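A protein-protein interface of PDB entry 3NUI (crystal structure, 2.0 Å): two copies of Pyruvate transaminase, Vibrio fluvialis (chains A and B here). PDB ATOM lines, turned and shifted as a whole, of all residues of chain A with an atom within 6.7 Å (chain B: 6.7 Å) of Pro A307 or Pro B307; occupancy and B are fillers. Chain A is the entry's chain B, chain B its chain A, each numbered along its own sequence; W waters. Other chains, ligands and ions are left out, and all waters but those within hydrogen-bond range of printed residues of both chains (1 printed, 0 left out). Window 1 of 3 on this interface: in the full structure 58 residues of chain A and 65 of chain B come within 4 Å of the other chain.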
ATOM      1  N   TYR A  90     -18.613 -33.286  16.967  1.00  0.00           N
ATOM      2  CA  TYR A  90     -17.260 -33.819  17.032  1.00  0.00           C
ATOM      3  C   TYR A  90     -17.258 -35.253  17.483  1.00  0.00           C
ATOM      4  O   TYR A  90     -16.455 -36.111  17.023  1.00  0.00           O
ATOM      5  CB  TYR A  90     -16.309 -32.890  17.855  1.00  0.00           C
ATOM      6  CG  TYR A  90     -15.843 -31.753  17.012  1.00  0.00           C
ATOM      7  CD1 TYR A  90     -14.693 -31.873  16.233  1.00  0.00           C
ATOM      8  CD2 TYR A  90     -16.606 -30.567  16.901  1.00  0.00           C
ATOM      9  CE1 TYR A  90     -14.291 -30.849  15.398  1.00  0.00           C
ATOM     10  CE2 TYR A  90     -16.188 -29.505  16.059  1.00  0.00           C
ATOM     11  CZ  TYR A  90     -15.047 -29.680  15.314  1.00  0.00           C
ATOM     12  OH  TYR A  90     -14.635 -28.681  14.509  1.00  0.00           O
ATOM     13  N   THR A 128     -18.725 -21.141   2.118  1.00  0.00           N
ATOM     14  CA  THR A 128     -17.362 -20.695   2.265  1.00  0.00           C
ATOM     15  C   THR A 128     -17.035 -20.789   3.758  1.00  0.00           C
ATOM     16  O   THR A 128     -17.885 -21.254   4.570  1.00  0.00           O
ATOM     17  CB  THR A 128     -17.252 -19.197   1.798  1.00  0.00           C
ATOM     18  OG1 THR A 128     -18.045 -18.395   2.660  1.00  0.00           O
ATOM     19  CG2 THR A 128     -17.781 -19.056   0.338  1.00  0.00           C
ATOM     20  N   ASN A 129     -15.832 -20.316   4.135  1.00  0.00           N
ATOM     21  CA  ASN A 129     -15.446 -20.302   5.551  1.00  0.00           C
ATOM     22  C   ASN A 129     -15.763 -19.020   6.260  1.00  0.00           C
ATOM     23  O   ASN A 129     -15.594 -18.964   7.483  1.00  0.00           O
ATOM     24  CB  ASN A 129     -13.980 -20.697   5.757  1.00  0.00           C
ATOM     25  CG  ASN A 129     -13.685 -22.074   5.208  1.00  0.00           C
ATOM     26  OD1 ASN A 129     -14.169 -23.053   5.731  1.00  0.00           O
ATOM     27  ND2 ASN A 129     -12.927 -22.142   4.114  1.00  0.00           N
ATOM     28  N   SER A 130     -16.248 -17.992   5.535  1.00  0.00           N
ATOM     29  CA  SER A 130     -16.550 -16.712   6.171  1.00  0.00           C
ATOM     30  C   SER A 130     -17.371 -15.822   5.254  1.00  0.00           C
ATOM     31  O   SER A 130     -17.427 -16.047   4.037  1.00  0.00           O
ATOM     32  CB  SER A 130     -15.270 -15.912   6.496  1.00  0.00           C
ATOM     33  OG  SER A 130     -14.548 -15.665   5.274  1.00  0.00           O
ATOM     34  N   SER A 298     -23.048 -14.835   6.792  1.00  0.00           N
ATOM     35  CA  SER A 298     -21.877 -15.290   7.477  1.00  0.00           C
ATOM     36  C   SER A 298     -21.870 -15.789   8.871  1.00  0.00           C
ATOM     37  O   SER A 298     -21.593 -16.925   9.081  1.00  0.00           O
ATOM     38  CB  SER A 298     -20.852 -14.221   7.506  1.00  0.00           C
ATOM     39  OG  SER A 298     -21.301 -13.124   8.239  1.00  0.00           O
ATOM     40  N   THR A 302     -23.981 -19.303  12.367  1.00  0.00           N
ATOM     41  CA  THR A 302     -23.669 -20.326  13.358  1.00  0.00           C
ATOM     42  C   THR A 302     -23.546 -19.722  14.765  1.00  0.00           C
ATOM     43  O   THR A 302     -23.008 -20.374  15.686  1.00  0.00           O
ATOM     44  CB  THR A 302     -22.341 -21.027  13.041  1.00  0.00           C
ATOM     45  OG1 THR A 302     -21.305 -20.067  13.125  1.00  0.00           O
ATOM     46  CG2 THR A 302     -22.360 -21.620  11.607  1.00  0.00           C
ATOM     47  N   GLY A 304     -21.605 -17.654  15.748  1.00  0.00           N
ATOM     48  CA  GLY A 304     -20.197 -17.527  16.109  1.00  0.00           C
ATOM     49  C   GLY A 304     -19.524 -18.827  16.531  1.00  0.00           C
ATOM     50  O   GLY A 304     -18.341 -18.804  16.889  1.00  0.00           O
ATOM     51  N   PHE A 305     -20.232 -19.961  16.471  1.00  0.00           N
ATOM     52  CA  PHE A 305     -19.659 -21.213  16.985  1.00  0.00           C
ATOM     53  C   PHE A 305     -18.753 -21.857  15.959  1.00  0.00           C
ATOM     54  O   PHE A 305     -17.967 -22.755  16.303  1.00  0.00           O
ATOM     55  CB  PHE A 305     -20.760 -22.237  17.459  1.00  0.00           C
ATOM     56  CG  PHE A 305     -21.315 -21.963  18.859  1.00  0.00           C
ATOM     57  CD1 PHE A 305     -21.863 -20.722  19.195  1.00  0.00           C
ATOM     58  CD2 PHE A 305     -21.272 -22.964  19.831  1.00  0.00           C
ATOM     59  CE1 PHE A 305     -22.372 -20.448  20.525  1.00  0.00           C
ATOM     60  CE2 PHE A 305     -21.775 -22.739  21.156  1.00  0.00           C
ATOM     61  CZ  PHE A 305     -22.312 -21.466  21.505  1.00  0.00           C
ATOM     62  N   PHE A 306     -18.865 -21.451  14.682  1.00  0.00           N
ATOM     63  CA  PHE A 306     -18.135 -22.178  13.629  1.00  0.00           C
ATOM     64  C   PHE A 306     -18.016 -21.287  12.399  1.00  0.00           C
ATOM     65  O   PHE A 306     -18.997 -20.741  11.942  1.00  0.00           O
ATOM     66  CB  PHE A 306     -18.857 -23.499  13.228  1.00  0.00           C
ATOM     67  CG  PHE A 306     -17.979 -24.506  12.461  1.00  0.00           C
ATOM     68  CD1 PHE A 306     -17.288 -25.516  13.136  1.00  0.00           C
ATOM     69  CD2 PHE A 306     -17.828 -24.411  11.079  1.00  0.00           C
ATOM     70  CE1 PHE A 306     -16.486 -26.456  12.438  1.00  0.00           C
ATOM     71  CE2 PHE A 306     -17.043 -25.356  10.339  1.00  0.00           C
ATOM     72  CZ  PHE A 306     -16.367 -26.374  11.002  1.00  0.00           C
ATOM     73  N   PRO A 307     -16.805 -21.207  11.830  1.00  0.00           N
ATOM     74  CA  PRO A 307     -16.573 -20.306  10.661  1.00  0.00           C
ATOM     75  C   PRO A 307     -17.296 -20.872   9.461  1.00  0.00           C
ATOM     76  O   PRO A 307     -16.997 -21.983   9.014  1.00  0.00           O
ATOM     77  CB  PRO A 307     -15.067 -20.399  10.392  1.00  0.00           C
ATOM     78  CG  PRO A 307     -14.499 -21.233  11.479  1.00  0.00           C
ATOM     79  CD  PRO A 307     -15.589 -21.930  12.243  1.00  0.00           C
ATOM     80  N   MET A 308     -18.210 -20.071   8.922  1.00  0.00           N
ATOM     81  CA  MET A 308     -18.876 -20.415   7.689  1.00  0.00           C
ATOM     82  C   MET A 308     -19.496 -19.204   7.089  1.00  0.00           C
ATOM     83  O   MET A 308     -19.888 -18.308   7.827  1.00  0.00           O
ATOM     84  CB  MET A 308     -19.954 -21.440   7.916  1.00  0.00           C
ATOM     85  CG  MET A 308     -20.075 -22.337   6.681  1.00  0.00           C
ATOM     86  SD  MET A 308     -20.887 -23.950   7.012  1.00  0.00           S
ATOM     87  CE  MET A 308     -22.313 -23.252   7.888  1.00  0.00           C
ATOM     88  N   GLY A 309     -19.558 -19.188   5.763  1.00  0.00           N
ATOM     89  CA  GLY A 309     -20.309 -18.157   5.025  1.00  0.00           C
ATOM     90  C   GLY A 309     -21.190 -18.849   4.010  1.00  0.00           C
ATOM     91  O   GLY A 309     -20.980 -20.044   3.689  1.00  0.00           O
ATOM     92  N   HIS A 340     -19.209 -27.207   5.113  1.00  0.00           N
ATOM     93  CA  HIS A 340     -18.609 -28.052   6.133  1.00  0.00           C
ATOM     94  C   HIS A 340     -19.717 -28.746   6.976  1.00  0.00           C
ATOM     95  O   HIS A 340     -20.599 -28.069   7.495  1.00  0.00           O
ATOM     96  CB  HIS A 340     -17.737 -27.174   7.069  1.00  0.00           C
ATOM     97  CG  HIS A 340     -16.797 -27.991   7.916  1.00  0.00           C
ATOM     98  ND1 HIS A 340     -17.236 -28.973   8.783  1.00  0.00           N
ATOM     99  CD2 HIS A 340     -15.445 -28.027   7.959  1.00  0.00           C
ATOM    100  CE1 HIS A 340     -16.195 -29.565   9.340  1.00  0.00           C
ATOM    101  NE2 HIS A 340     -15.097 -29.014   8.862  1.00  0.00           N
ATOM    102  N   GLY A 343     -20.176 -27.395  10.567  1.00  0.00           N
ATOM    103  CA  GLY A 343     -20.768 -26.060  10.418  1.00  0.00           C
ATOM    104  C   GLY A 343     -22.213 -26.058  10.036  1.00  0.00           C
ATOM    105  O   GLY A 343     -22.977 -25.302  10.608  1.00  0.00           O
ATOM    106  N   TYR B  90     -15.388 -26.177  23.276  1.00  0.00           N
ATOM    107  CA  TYR B  90     -16.773 -25.688  23.156  1.00  0.00           C
ATOM    108  C   TYR B  90     -17.403 -25.498  24.563  1.00  0.00           C
ATOM    109  O   TYR B  90     -18.212 -24.623  24.806  1.00  0.00           O
ATOM    110  CB  TYR B  90     -17.609 -26.657  22.294  1.00  0.00           C
ATOM    111  CG  TYR B  90     -17.535 -26.316  20.802  1.00  0.00           C
ATOM    112  CD1 TYR B  90     -18.029 -25.111  20.334  1.00  0.00           C
ATOM    113  CD2 TYR B  90     -16.898 -27.178  19.884  1.00  0.00           C
ATOM    114  CE1 TYR B  90     -17.940 -24.760  18.943  1.00  0.00           C
ATOM    115  CE2 TYR B  90     -16.847 -26.879  18.504  1.00  0.00           C
ATOM    116  CZ  TYR B  90     -17.330 -25.664  18.057  1.00  0.00           C
ATOM    117  OH  TYR B  90     -17.292 -25.357  16.731  1.00  0.00           O
ATOM    118  N   THR B 128      -6.742 -16.452  10.589  1.00  0.00           N
ATOM    119  CA  THR B 128      -7.806 -16.237   9.612  1.00  0.00           C
ATOM    120  C   THR B 128      -8.609 -17.530   9.611  1.00  0.00           C
ATOM    121  O   THR B 128      -8.308 -18.456  10.354  1.00  0.00           O
ATOM    122  CB  THR B 128      -7.265 -16.025   8.161  1.00  0.00           C
ATOM    123  OG1 THR B 128      -6.577 -17.201   7.757  1.00  0.00           O
ATOM    124  CG2 THR B 128      -6.238 -14.864   8.032  1.00  0.00           C
ATOM    125  N   ASN B 129      -9.635 -17.589   8.748  1.00  0.00           N
ATOM    126  CA  ASN B 129     -10.412 -18.798   8.612  1.00  0.00           C
ATOM    127  C   ASN B 129      -9.925 -19.808   7.642  1.00  0.00           C
ATOM    128  O   ASN B 129     -10.518 -20.876   7.634  1.00  0.00           O
ATOM    129  CB  ASN B 129     -11.897 -18.484   8.292  1.00  0.00           C
ATOM    130  CG  ASN B 129     -12.496 -17.604   9.363  1.00  0.00           C
ATOM    131  OD1 ASN B 129     -12.667 -18.057  10.491  1.00  0.00           O
ATOM    132  ND2 ASN B 129     -12.694 -16.287   9.055  1.00  0.00           N
ATOM    133  N   SER B 130      -8.917 -19.498   6.814  1.00  0.00           N
ATOM    134  CA  SER B 130      -8.491 -20.445   5.773  1.00  0.00           C
ATOM    135  C   SER B 130      -7.166 -20.013   5.189  1.00  0.00           C
ATOM    136  O   SER B 130      -6.716 -18.857   5.331  1.00  0.00           O
ATOM    137  CB  SER B 130      -9.512 -20.481   4.591  1.00  0.00           C
ATOM    138  OG  SER B 130      -9.422 -19.192   3.922  1.00  0.00           O
ATOM    139  N   SER B 298      -2.313 -23.690   7.585  1.00  0.00           N
ATOM    140  CA  SER B 298      -3.729 -24.151   7.527  1.00  0.00           C
ATOM    141  C   SER B 298      -3.871 -25.738   7.523  1.00  0.00           C
ATOM    142  O   SER B 298      -2.900 -26.306   7.901  1.00  0.00           O
ATOM    143  CB  SER B 298      -4.472 -23.433   6.416  1.00  0.00           C
ATOM    144  OG  SER B 298      -5.797 -23.716   6.435  1.00  0.00           O
ATOM    145  N   THR B 302      -4.804 -27.795  12.133  1.00  0.00           N
ATOM    146  CA  THR B 302      -5.867 -28.261  13.031  1.00  0.00           C
ATOM    147  C   THR B 302      -6.128 -29.772  12.800  1.00  0.00           C
ATOM    148  O   THR B 302      -7.118 -30.324  13.300  1.00  0.00           O
ATOM    149  CB  THR B 302      -7.189 -27.472  12.775  1.00  0.00           C
ATOM    150  OG1 THR B 302      -7.581 -27.620  11.387  1.00  0.00           O
ATOM    151  CG2 THR B 302      -6.959 -25.942  13.072  1.00  0.00           C
ATOM    152  N   GLY B 304      -7.158 -30.999  10.335  1.00  0.00           N
ATOM    153  CA  GLY B 304      -8.394 -31.109   9.516  1.00  0.00           C
ATOM    154  C   GLY B 304      -9.699 -31.000  10.338  1.00  0.00           C
ATOM    155  O   GLY B 304     -10.769 -31.031   9.764  1.00  0.00           O
ATOM    156  N   PHE B 305      -9.588 -30.807  11.653  1.00  0.00           N
ATOM    157  CA  PHE B 305     -10.777 -30.857  12.542  1.00  0.00           C
ATOM    158  C   PHE B 305     -11.462 -29.501  12.684  1.00  0.00           C
ATOM    159  O   PHE B 305     -12.545 -29.436  13.270  1.00  0.00           O
ATOM    160  CB  PHE B 305     -10.393 -31.455  13.912  1.00  0.00           C
ATOM    161  CG  PHE B 305     -10.362 -32.958  13.899  1.00  0.00           C
ATOM    162  CD1 PHE B 305      -9.150 -33.643  13.780  1.00  0.00           C
ATOM    163  CD2 PHE B 305     -11.562 -33.694  13.955  1.00  0.00           C
ATOM    164  CE1 PHE B 305      -9.130 -35.040  13.782  1.00  0.00           C
ATOM    165  CE2 PHE B 305     -11.568 -35.063  13.892  1.00  0.00           C
ATOM    166  CZ  PHE B 305     -10.347 -35.743  13.832  1.00  0.00           C
ATOM    167  N   PHE B 306     -10.857 -28.435  12.114  1.00  0.00           N
ATOM    168  CA  PHE B 306     -11.446 -27.104  12.225  1.00  0.00           C
ATOM    169  C   PHE B 306     -10.840 -26.142  11.152  1.00  0.00           C
ATOM    170  O   PHE B 306      -9.621 -26.116  10.976  1.00  0.00           O
ATOM    171  CB  PHE B 306     -11.136 -26.530  13.635  1.00  0.00           C
ATOM    172  CG  PHE B 306     -12.075 -25.396  14.060  1.00  0.00           C
ATOM    173  CD1 PHE B 306     -13.201 -25.668  14.844  1.00  0.00           C
ATOM    174  CD2 PHE B 306     -11.836 -24.088  13.641  1.00  0.00           C
ATOM    175  CE1 PHE B 306     -14.113 -24.577  15.208  1.00  0.00           C
ATOM    176  CE2 PHE B 306     -12.667 -23.044  13.999  1.00  0.00           C
ATOM    177  CZ  PHE B 306     -13.786 -23.265  14.817  1.00  0.00           C
ATOM    178  N   PRO B 307     -11.681 -25.366  10.467  1.00  0.00           N
ATOM    179  CA  PRO B 307     -11.140 -24.486   9.428  1.00  0.00           C
ATOM    180  C   PRO B 307     -10.453 -23.299  10.097  1.00  0.00           C
ATOM    181  O   PRO B 307     -11.079 -22.484  10.807  1.00  0.00           O
ATOM    182  CB  PRO B 307     -12.360 -24.051   8.591  1.00  0.00           C
ATOM    183  CG  PRO B 307     -13.501 -24.874   9.164  1.00  0.00           C
ATOM    184  CD  PRO B 307     -13.133 -25.260  10.575  1.00  0.00           C
ATOM    185  N   MET B 308      -9.149 -23.254   9.925  1.00  0.00           N
ATOM    186  CA  MET B 308      -8.416 -22.053  10.385  1.00  0.00           C
ATOM    187  C   MET B 308      -7.140 -21.855   9.590  1.00  0.00           C
ATOM    188  O   MET B 308      -6.606 -22.798   9.079  1.00  0.00           O
ATOM    189  CB  MET B 308      -8.128 -22.129  11.890  1.00  0.00           C
ATOM    190  CG  MET B 308      -7.883 -20.740  12.525  1.00  0.00           C
ATOM    191  SD  MET B 308      -7.856 -20.831  14.387  1.00  0.00           S
ATOM    192  CE  MET B 308      -6.285 -21.671  14.516  1.00  0.00           C
ATOM    193  N   GLY B 309      -6.694 -20.597   9.469  1.00  0.00           N
ATOM    194  CA  GLY B 309      -5.427 -20.244   8.877  1.00  0.00           C
ATOM    195  C   GLY B 309      -4.576 -19.538   9.951  1.00  0.00           C
ATOM    196  O   GLY B 309      -5.112 -18.995  10.935  1.00  0.00           O
ATOM    197  N   GLY B 339      -8.950 -15.961  13.858  1.00  0.00           N
ATOM    198  CA  GLY B 339      -9.310 -17.374  13.784  1.00  0.00           C
ATOM    199  C   GLY B 339     -10.460 -17.622  14.753  1.00  0.00           C
ATOM    200  O   GLY B 339     -11.493 -16.922  14.669  1.00  0.00           O
ATOM    201  N   HIS B 340     -10.327 -18.587  15.660  1.00  0.00           N
ATOM    202  CA  HIS B 340     -11.483 -18.893  16.567  1.00  0.00           C
ATOM    203  C   HIS B 340     -10.872 -19.638  17.746  1.00  0.00           C
ATOM    204  O   HIS B 340      -9.948 -20.363  17.532  1.00  0.00           O
ATOM    205  CB  HIS B 340     -12.419 -19.820  15.794  1.00  0.00           C
ATOM    206  CG  HIS B 340     -13.726 -20.076  16.451  1.00  0.00           C
ATOM    207  ND1 HIS B 340     -13.869 -20.976  17.477  1.00  0.00           N
ATOM    208  CD2 HIS B 340     -14.975 -19.627  16.159  1.00  0.00           C
ATOM    209  CE1 HIS B 340     -15.148 -21.072  17.798  1.00  0.00           C
ATOM    210  NE2 HIS B 340     -15.843 -20.266  17.016  1.00  0.00           N
ATOM    211  N   GLY B 343     -10.809 -23.367  17.125  1.00  0.00           N
ATOM    212  CA  GLY B 343      -9.718 -23.683  16.133  1.00  0.00           C
ATOM    213  C   GLY B 343      -8.351 -23.658  16.829  1.00  0.00           C
ATOM    214  O   GLY B 343      -7.480 -24.527  16.590  1.00  0.00           O
HETATM  215  O   HOH W   1     -12.384 -28.966   9.718  1.00  0.00           O
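The side-chain hydroxyl (OH) of Tyr B90 lies within hydrogen-bond range of the backbone carbonyl oxygen (O) of Phe A305, at 2.7 Å.
OH of Tyr A90 lies within hydrogen-bond range of O of Phe B305 (2.5 Å).
The backbone carbonyl oxygen (O) of Gly A304 is in hydrogen-bond range of a ring nitrogen (NE2) of His B340 (2.9 Å).
O of Phe A305 lies within hydrogen-bond range of NE2 of His B340 (3.3 Å).
Of the 14 printed residues of chain A, 8 touch a printed residue of chain B.
Printed residues of chain A that touch a printed residue of chain B: Tyr A90, Asn A129, Ser A130, Gly A304, Phe A305, Phe A306, Pro A307 and His A340.
Hydrophobic or aromatic side chains of chain A within 4 Å of the printed part of chain B: Tyr A90, Phe A305, Phe A306, Pro A307 and His A340.
Hydrophobic or aromatic side chains of chain B within 4 Å of the printed part of chain A: Tyr B90, Phe B306, Pro B307 and His B340.
Among the printed residues, 18 pairs touch across the chains.
Water W1 lies within hydrogen-bond range of the backbone carbonyl oxygen of Gly B304 (2.6 Å), a ring nitrogen (NE2) of His A340 (2.8 Å) and the backbone NH of Phe B306 (2.9 Å).
Pro A307 touches just these residues of chain B: Asn B129, Phe B306 and Pro B307.
Pro B307 touches just these residues of chain A: Asn A129, Phe A306, Pro A307 and His A340.
Of the printed residues of chain B, His A340 touches Pro B307 (3.9 Å).
Of the printed residues of chain A, Asn B129 touches Asn A129, Ser A130 and Pro A307.
Printed residues of chain A within 4 Å of Ser B130: Asn A129.
Gly A309 touches none of the printed residues of chain B.
The nearest residue of chain B that does not touch Pro A307 is His B340 (4.6 Å).
The nearest printed residue of chain B that does not touch Gly A304 is Tyr B90 (6.3 Å).
Tyr A90 touches Phe B305, and with the chains exchanged Phe A305 touches Tyr B90.
Tyr A90 touches Phe B306, and with the chains exchanged Phe A306 touches Tyr B90.
Asn A129 touches its own counterpart, Asn B129.
Phe A306 touches Pro B307, and with the chains exchanged Pro A307 touches Phe B306.
Positions printed for both chains: 90, 128, 129, 130, 298, 302, 304, 305, 306, 307, 308, 309, 340 and 343.
Of the 18 pairs that touch across the chains among the printed residues, 14 have their exchanged pair printed and touching as well.
CD1 of Phe B306 touches OH of Tyr A90, 3.4 Å away.
Asn B129 touches Asn A129 (CB to O, 3.8 Å).
ND2 of Asn B129 touches CB of Ser A130, 3.7 Å away.
Tyr B90 touches Phe A306 (OH to CD1, 3.6 Å).
Phe A306 touches Phe B306 (CD1 to CE1, 3.9 Å).
Pro B307 touches Phe A306.
His B340 touches Phe A306 (NE2 to N, 3.998 Å).
CD of Pro A307 touches CZ of Phe B306, at 3.4 Å.
CG of Pro A307 touches O of Pro B307, at 3.7 Å.
His A340 touches Pro B307 (CD2 to CG, 3.9 Å).
The backbone carbonyl oxygen (O) of Ser B130 sits at hydrogen-bond distance from the side-chain hydroxyl (OG1) of Thr B128.
O of Phe B306 is in hydrogen-bond range of OG1 of Thr B302.
SD of Met B308 lies within hydrogen-bond range of N of His B340 (3.6 Å).
The side-chain hydroxyl (OG1) of Thr A128 lies within hydrogen-bond range of the backbone carbonyl oxygen (O) of Ser A130.
N of Met A308 is in hydrogen-bond range of O of Asn A129 (3.2 Å).
The side-chain hydroxyl (OG1) of Thr A302 sits at hydrogen-bond distance from the backbone carbonyl oxygen (O) of Phe A306 (2.7 Å).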
